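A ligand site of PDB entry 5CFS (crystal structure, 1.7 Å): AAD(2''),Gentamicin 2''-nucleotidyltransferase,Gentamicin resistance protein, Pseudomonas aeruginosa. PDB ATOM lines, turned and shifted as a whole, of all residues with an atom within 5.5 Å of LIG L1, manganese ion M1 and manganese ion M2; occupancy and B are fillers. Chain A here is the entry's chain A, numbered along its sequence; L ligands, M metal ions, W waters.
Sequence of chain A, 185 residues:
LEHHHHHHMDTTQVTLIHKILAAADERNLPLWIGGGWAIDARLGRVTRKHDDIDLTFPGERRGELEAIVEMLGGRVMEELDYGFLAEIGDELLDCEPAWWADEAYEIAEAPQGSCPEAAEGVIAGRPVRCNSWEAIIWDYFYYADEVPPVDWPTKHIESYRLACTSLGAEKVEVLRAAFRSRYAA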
ATOM      1  N   GLY A  35      -7.337  23.848 -31.187  1.00  0.00           N
ATOM      2  CA  GLY A  35      -8.004  24.361 -32.367  1.00  0.00           C
ATOM      3  C   GLY A  35      -7.320  24.040 -33.678  1.00  0.00           C
ATOM      4  O   GLY A  35      -6.796  22.942 -33.882  1.00  0.00           O
ATOM      5  N   GLY A  36      -7.317  25.008 -34.583  1.00  0.00           N
ATOM      6  CA  GLY A  36      -6.841  24.774 -35.926  1.00  0.00           C
ATOM      7  C   GLY A  36      -5.389  24.380 -35.984  1.00  0.00           C
ATOM      8  O   GLY A  36      -5.023  23.489 -36.755  1.00  0.00           O
ATOM      9  N   ASP A  52      -5.915  32.672 -35.282  1.00  0.00           N
ATOM     10  CA  ASP A  52      -5.303  32.837 -33.965  1.00  0.00           C
ATOM     11  C   ASP A  52      -4.508  31.597 -33.586  1.00  0.00           C
ATOM     12  O   ASP A  52      -4.395  30.654 -34.367  1.00  0.00           O
ATOM     13  CB  ASP A  52      -6.363  33.173 -32.886  1.00  0.00           C
ATOM     14  CG  ASP A  52      -7.356  32.038 -32.636  1.00  0.00           C
ATOM     15  OD1 ASP A  52      -7.070  30.897 -33.023  1.00  0.00           O
ATOM     16  OD2 ASP A  52      -8.416  32.277 -32.017  1.00  0.00           O
ATOM     17  N   ILE A  53      -3.944  31.625 -32.384  1.00  0.00           N
ATOM     18  CA  ILE A  53      -3.298  30.456 -31.794  1.00  0.00           C
ATOM     19  C   ILE A  53      -4.094  30.112 -30.547  1.00  0.00           C
ATOM     20  O   ILE A  53      -4.202  30.931 -29.625  1.00  0.00           O
ATOM     21  CB  ILE A  53      -1.822  30.724 -31.426  1.00  0.00           C
ATOM     22  CG1 ILE A  53      -1.009  31.090 -32.667  1.00  0.00           C
ATOM     23  CG2 ILE A  53      -1.220  29.492 -30.763  1.00  0.00           C
ATOM     24  CD1 ILE A  53       0.315  31.758 -32.349  1.00  0.00           C
ATOM     25  N   ASP A  54      -4.675  28.910 -30.521  1.00  0.00           N
ATOM     26  CA  ASP A  54      -5.429  28.456 -29.350  1.00  0.00           C
ATOM     27  C   ASP A  54      -4.495  27.679 -28.437  1.00  0.00           C
ATOM     28  O   ASP A  54      -3.799  26.768 -28.884  1.00  0.00           O
ATOM     29  CB  ASP A  54      -6.612  27.583 -29.762  1.00  0.00           C
ATOM     30  CG  ASP A  54      -7.578  28.286 -30.683  1.00  0.00           C
ATOM     31  OD1 ASP A  54      -8.266  29.228 -30.239  1.00  0.00           O
ATOM     32  OD2 ASP A  54      -7.652  27.904 -31.866  1.00  0.00           O
ATOM     33  N   TYR A  82     -14.455  31.336 -20.694  1.00  0.00           N
ATOM     34  CA  TYR A  82     -13.721  30.066 -20.616  1.00  0.00           C
ATOM     35  C   TYR A  82     -12.232  30.256 -20.380  1.00  0.00           C
ATOM     36  O   TYR A  82     -11.532  29.273 -20.169  1.00  0.00           O
ATOM     37  CB  TYR A  82     -13.910  29.264 -21.905  1.00  0.00           C
ATOM     38  CG  TYR A  82     -13.410  29.994 -23.128  1.00  0.00           C
ATOM     39  CD1 TYR A  82     -12.067  29.987 -23.466  1.00  0.00           C
ATOM     40  CD2 TYR A  82     -14.291  30.698 -23.943  1.00  0.00           C
ATOM     41  CE1 TYR A  82     -11.606  30.659 -24.560  1.00  0.00           C
ATOM     42  CE2 TYR A  82     -13.835  31.371 -25.059  1.00  0.00           C
ATOM     43  CZ  TYR A  82     -12.500  31.349 -25.360  1.00  0.00           C
ATOM     44  OH  TYR A  82     -12.067  32.019 -26.472  1.00  0.00           O
ATOM     45  N   ASP A  94      -5.547  32.650 -27.835  1.00  0.00           N
ATOM     46  CA  ASP A  94      -6.836  32.317 -27.267  1.00  0.00           C
ATOM     47  C   ASP A  94      -6.622  31.222 -26.229  1.00  0.00           C
ATOM     48  O   ASP A  94      -6.436  30.054 -26.582  1.00  0.00           O
ATOM     49  CB  ASP A  94      -7.760  31.882 -28.408  1.00  0.00           C
ATOM     50  CG  ASP A  94      -9.152  31.557 -27.959  1.00  0.00           C
ATOM     51  OD1 ASP A  94      -9.484  31.703 -26.766  1.00  0.00           O
ATOM     52  OD2 ASP A  94      -9.942  31.176 -28.850  1.00  0.00           O
ATOM     53  N   GLU A  96      -7.147  28.863 -22.745  1.00  0.00           N
ATOM     54  CA  GLU A  96      -8.077  28.210 -21.844  1.00  0.00           C
ATOM     55  C   GLU A  96      -7.339  27.413 -20.776  1.00  0.00           C
ATOM     56  O   GLU A  96      -6.388  26.684 -21.081  1.00  0.00           O
ATOM     57  CB  GLU A  96      -9.017  27.283 -22.626  1.00  0.00           C
ATOM     58  CG  GLU A  96     -10.062  26.597 -21.749  1.00  0.00           C
ATOM     59  CD  GLU A  96     -11.061  25.764 -22.544  1.00  0.00           C
ATOM     60  OE1 GLU A  96     -10.692  25.268 -23.627  1.00  0.00           O
ATOM     61  OE2 GLU A  96     -12.229  25.639 -22.074  1.00  0.00           O
ATOM     62  N   ILE A 107      -9.140  19.859 -19.541  1.00  0.00           N
ATOM     63  CA  ILE A 107     -10.022  20.970 -19.856  1.00  0.00           C
ATOM     64  C   ILE A 107     -11.376  20.714 -19.232  1.00  0.00           C
ATOM     65  O   ILE A 107     -11.885  19.582 -19.304  1.00  0.00           O
ATOM     66  CB  ILE A 107     -10.165  21.149 -21.380  1.00  0.00           C
ATOM     67  CG1 ILE A 107      -8.851  21.641 -21.984  1.00  0.00           C
ATOM     68  CG2 ILE A 107     -11.295  22.120 -21.726  1.00  0.00           C
ATOM     69  CD1 ILE A 107      -8.772  21.491 -23.472  1.00  0.00           C
ATOM     70  N   ALA A 108     -11.965  21.733 -18.607  1.00  0.00           N
ATOM     71  CA  ALA A 108     -13.259  21.564 -17.967  1.00  0.00           C
ATOM     72  C   ALA A 108     -14.287  21.020 -18.951  1.00  0.00           C
ATOM     73  O   ALA A 108     -14.379  21.481 -20.082  1.00  0.00           O
ATOM     74  CB  ALA A 108     -13.742  22.894 -17.388  1.00  0.00           C
ATOM     75  N   GLU A 109     -15.010  19.992 -18.513  1.00  0.00           N
ATOM     76  CA  GLU A 109     -16.132  19.391 -19.249  1.00  0.00           C
ATOM     77  C   GLU A 109     -15.713  18.560 -20.466  1.00  0.00           C
ATOM     78  O   GLU A 109     -16.562  17.901 -21.075  1.00  0.00           O
ATOM     79  CB  GLU A 109     -17.133  20.469 -19.692  1.00  0.00           C
ATOM     80  CG  GLU A 109     -17.876  21.142 -18.528  1.00  0.00           C
ATOM     81  CD  GLU A 109     -19.364  20.828 -18.530  1.00  0.00           C
ATOM     82  OE1 GLU A 109     -20.174  21.756 -18.735  1.00  0.00           O
ATOM     83  OE2 GLU A 109     -19.725  19.648 -18.329  1.00  0.00           O
ATOM     84  N   ALA A 110     -14.428  18.558 -20.819  1.00  0.00           N
ATOM     85  CA  ALA A 110     -13.973  17.830 -22.014  1.00  0.00           C
ATOM     86  C   ALA A 110     -13.798  16.345 -21.713  1.00  0.00           C
ATOM     87  O   ALA A 110     -13.763  15.934 -20.549  1.00  0.00           O
ATOM     88  CB  ALA A 110     -12.677  18.421 -22.515  1.00  0.00           C
ATOM     89  N   ASP A 139     -15.217  20.557 -29.066  1.00  0.00           N
ATOM     90  CA  ASP A 139     -15.550  21.970 -29.146  1.00  0.00           C
ATOM     91  C   ASP A 139     -16.444  22.293 -30.337  1.00  0.00           C
ATOM     92  O   ASP A 139     -17.195  23.264 -30.282  1.00  0.00           O
ATOM     93  CB  ASP A 139     -14.274  22.827 -29.181  1.00  0.00           C
ATOM     94  CG  ASP A 139     -13.776  23.183 -27.786  1.00  0.00           C
ATOM     95  OD1 ASP A 139     -14.542  22.980 -26.815  1.00  0.00           O
ATOM     96  OD2 ASP A 139     -12.641  23.683 -27.665  1.00  0.00           O
ATOM     97  N   TYR A 142     -20.144  21.984 -29.155  1.00  0.00           N
ATOM     98  CA  TYR A 142     -20.654  23.217 -28.555  1.00  0.00           C
ATOM     99  C   TYR A 142     -21.062  24.229 -29.613  1.00  0.00           C
ATOM    100  O   TYR A 142     -22.095  24.886 -29.515  1.00  0.00           O
ATOM    101  CB  TYR A 142     -19.615  23.883 -27.655  1.00  0.00           C
ATOM    102  CG  TYR A 142     -19.310  23.160 -26.368  1.00  0.00           C
ATOM    103  CD1 TYR A 142     -20.264  23.023 -25.384  1.00  0.00           C
ATOM    104  CD2 TYR A 142     -18.033  22.675 -26.129  1.00  0.00           C
ATOM    105  CE1 TYR A 142     -19.970  22.390 -24.203  1.00  0.00           C
ATOM    106  CE2 TYR A 142     -17.725  22.045 -24.964  1.00  0.00           C
ATOM    107  CZ  TYR A 142     -18.693  21.909 -24.005  1.00  0.00           C
ATOM    108  OH  TYR A 142     -18.401  21.285 -22.823  1.00  0.00           O
HETATM  109  C1  LIG L   1     -16.021  25.526 -25.265  1.00  0.00           C
HETATM  110  O1  LIG L   1     -15.185  26.652 -25.317  1.00  0.00           O
HETATM  111  C2  LIG L   1     -17.453  26.027 -25.135  1.00  0.00           C
HETATM  112  N1  LIG L   1     -17.788  26.951 -26.238  1.00  0.00           N
HETATM  113  C3  LIG L   1     -17.611  26.686 -23.779  1.00  0.00           C
HETATM  114  C4  LIG L   1     -17.231  25.745 -22.646  1.00  0.00           C
HETATM  115  O2  LIG L   1     -17.310  26.414 -21.392  1.00  0.00           O
HETATM  116  C5  LIG L   1     -15.807  25.241 -22.861  1.00  0.00           C
HETATM  117  O3  LIG L   1     -15.657  24.679 -24.186  1.00  0.00           O
HETATM  118  C6  LIG L   1     -15.451  24.167 -21.856  1.00  0.00           C
HETATM  119  N2  LIG L   1     -14.135  23.567 -22.059  1.00  0.00           N
HETATM  120  C7  LIG L   1     -11.807  28.178 -27.154  1.00  0.00           C
HETATM  121  N3  LIG L   1     -10.647  28.502 -28.007  1.00  0.00           N
HETATM  122  C8  LIG L   1     -11.694  26.753 -26.612  1.00  0.00           C
HETATM  123  C9  LIG L   1     -12.860  26.450 -25.664  1.00  0.00           C
HETATM  124  N4  LIG L   1     -12.789  25.058 -25.212  1.00  0.00           N
HETATM  125  C10 LIG L   1     -14.196  26.688 -26.356  1.00  0.00           C
HETATM  126  C11 LIG L   1     -14.305  28.064 -27.008  1.00  0.00           C
HETATM  127  O4  LIG L   1     -15.509  28.112 -27.763  1.00  0.00           O
HETATM  128  C12 LIG L   1     -13.116  28.286 -27.929  1.00  0.00           C
HETATM  129  O5  LIG L   1     -13.231  29.609 -28.464  1.00  0.00           O
HETATM  130  C13 LIG L   1     -13.957  29.722 -29.659  1.00  0.00           C
HETATM  131  C14 LIG L   1     -13.012  30.271 -30.727  1.00  0.00           C
HETATM  132  O6  LIG L   1     -11.860  29.436 -30.816  1.00  0.00           O
HETATM  133  C15 LIG L   1     -12.580  31.690 -30.367  1.00  0.00           C
HETATM  134  N5  LIG L   1     -11.680  32.239 -31.384  1.00  0.00           N
HETATM  135  C16 LIG L   1     -13.842  32.536 -30.222  1.00  0.00           C
HETATM  136  O7  LIG L   1     -13.482  33.865 -29.871  1.00  0.00           O
HETATM  137  C17 LIG L   1     -14.706  31.923 -29.121  1.00  0.00           C
HETATM  138  O8  LIG L   1     -15.062  30.574 -29.483  1.00  0.00           O
HETATM  139  C18 LIG L   1     -15.991  32.656 -28.891  1.00  0.00           C
HETATM  140  O9  LIG L   1     -16.789  32.002 -27.903  1.00  0.00           O
HETATM  141  P1  LG2 L   2      -8.048  29.089 -37.023  1.00  0.00           P
HETATM  142  O1  LG2 L   2      -8.174  29.909 -38.241  1.00  0.00           O
HETATM  143  O2  LG2 L   2      -8.196  29.907 -35.726  1.00  0.00           O
HETATM  144  O3  LG2 L   2      -6.794  28.297 -36.893  1.00  0.00           O
HETATM  145  P2  LG2 L   2      -9.975  27.400 -35.746  1.00  0.00           P
HETATM  146  O4  LG2 L   2     -10.457  25.985 -36.003  1.00  0.00           O
HETATM  147  O5  LG2 L   2      -8.979  27.372 -34.542  1.00  0.00           O
HETATM  148  O6  LG2 L   2      -9.183  27.966 -36.986  1.00  0.00           O
HETATM  149  P3  LG2 L   2     -11.536  29.269 -33.795  1.00  0.00           P
HETATM  150  O7  LG2 L   2     -12.323  30.558 -33.728  1.00  0.00           O
HETATM  151  O8  LG2 L   2     -10.156  29.607 -33.141  1.00  0.00           O
HETATM  152  C1  LG2 L   2     -11.237  28.657 -35.453  1.00  0.00           C
HETATM  153  O9  LG2 L   2     -12.203  28.146 -32.917  1.00  0.00           O
HETATM  154  C2  LG2 L   2     -12.008  26.733 -33.134  1.00  0.00           C
HETATM  155  C3  LG2 L   2     -12.970  25.968 -32.265  1.00  0.00           C
HETATM  156  O10 LG2 L   2     -13.859  26.890 -31.575  1.00  0.00           O
HETATM  157  C4  LG2 L   2     -13.885  25.010 -33.014  1.00  0.00           C
HETATM  158  O11 LG2 L   2     -14.262  23.918 -32.181  1.00  0.00           O
HETATM  159  C5  LG2 L   2     -15.099  25.892 -33.289  1.00  0.00           C
HETATM  160  O12 LG2 L   2     -16.270  25.124 -33.517  1.00  0.00           O
HETATM  161  C6  LG2 L   2     -15.194  26.634 -31.967  1.00  0.00           C
HETATM  162  N1  LG2 L   2     -15.927  27.893 -32.046  1.00  0.00           N
HETATM  163  C7  LG2 L   2     -15.752  28.905 -32.952  1.00  0.00           C
HETATM  164  N2  LG2 L   2     -16.605  29.898 -32.837  1.00  0.00           N
HETATM  165  C8  LG2 L   2     -17.397  29.500 -31.773  1.00  0.00           C
HETATM  166  C9  LG2 L   2     -18.522  30.096 -31.166  1.00  0.00           C
HETATM  167  N3  LG2 L   2     -19.033  31.281 -31.530  1.00  0.00           N
HETATM  168  N4  LG2 L   2     -19.117  29.425 -30.148  1.00  0.00           N
HETATM  169  C10 LG2 L   2     -18.599  28.250 -29.770  1.00  0.00           C
HETATM  170  N5  LG2 L   2     -17.545  27.603 -30.256  1.00  0.00           N
HETATM  171  C11 LG2 L   2     -16.992  28.279 -31.274  1.00  0.00           C
HETATM  172 MN    MN M   1      -8.117  29.135 -33.598  1.00  0.00          MN
HETATM  173 MN    MN M   2      -9.644  30.729 -31.060  1.00  0.00          MN
HETATM  174  O   HOH W   1     -16.721  25.458 -28.654  1.00  0.00           O
HETATM  175  O   HOH W   2     -17.523  29.769 -25.375  1.00  0.00           O
HETATM  176  O   HOH W   3      -8.352  28.210 -26.311  1.00  0.00           O
HETATM  177  O   HOH W   4     -15.124  26.400 -18.834  1.00  0.00           O
HETATM  178  O   HOH W   5     -20.459  27.263 -26.227  1.00  0.00           O
HETATM  179  O   HOH W   6     -13.954  22.042 -24.388  1.00  0.00           O
HETATM  180  O   HOH W   7      -6.102  28.550 -34.492  1.00  0.00           O
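The side-chain carboxylate (OD1) of Asp 94 is in hydrogen-bond range of the side-chain hydroxyl (OH) of Tyr 82, at 2.6 Å.
The backbone carbonyl oxygen (O) of Ile 53 lies within hydrogen-bond range of the backbone NH (N) of Asp 94, 2.8 Å away.
The side-chain carboxylate of Glu 96 is in salt-bridge range of a nitrogen (N4) of LIG L1, at 2.6 Å.
The side-chain carboxylate (OD2) of Asp 139 lies within salt-bridge range of a nitrogen (N4) of LIG L1 (2.8 Å).
The backbone carbonyl oxygen (O) of Ala 108 sits at hydrogen-bond distance from a nitrogen (N2) of LIG L1 (2.9 Å).
OH of Tyr 82 sits at hydrogen-bond distance from O5 of LIG L1.
The backbone NH (N) of Gly 36 lies close to an oxygen (O5) of LG2 L2, 2.9 Å away.
Merely in contact with LIG L1: Ile 107 (3.2 Å) and Tyr 142 (3.4 Å).
Hydrophobic or aromatic side chains within 4 Å of LIG L1: Tyr 82, Ile 107 and Tyr 142.
Of the 14 residues printed, 9 come within 4 Å of LIG L1.
Manganese ion M1 is bound by the side-chain carboxylate of Asp 52 (2.1 Å), an oxygen (O8) of LG2 L2 (2.1 Å), the side-chain carboxylate of Asp 54 (2.2 Å), an oxygen (O5) of LG2 L2 (2.2 Å), an oxygen (O2) of LG2 L2 (2.3 Å) and water W7 (2.3 Å).
Manganese ion M1 has six donor atoms within binding distance.
Water W7 lies within hydrogen-bond range of O3 of LG2 L2 (2.5 Å) and O of Asp 52 (2.7 Å).
Water W6 lies within hydrogen-bond range of OD1 of Asp 139 and N2 of LIG L1.
Water W3 bridges O of Asp 94 (2.7 Å) and N3 of LIG L1 (2.9 Å).
Water W1 lies within hydrogen-bond range of O of Asp 139 (2.8 Å), N5 of LG2 L2 (2.8 Å) and N1 of LIG L1 (3.0 Å).
Three residues have an atom within 4 Å of manganese ion M2: Asp 52, Asp 54 and Asp 94.
Along chain A the residues within 4 Å of manganese ion M2 span positions 52 to 94.
The nearest printed residue that does not touch manganese ion M2 is Tyr 82 (5.3 Å).
Manganese ion M2 is bound by OD2 of Asp 52 (2.2 Å), OD1 of Asp 54 (2.2 Å), OD2 of Asp 94 (2.3 Å), O8 of LG2 L2 (2.4 Å), N5 of LIG L1 (2.6 Å) and O6 of LIG L1 (2.6 Å).
Manganese ion M2 has six donor atoms within binding distance.
Of the 14 residues printed, 2 come within 4 Å of manganese ion M1.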
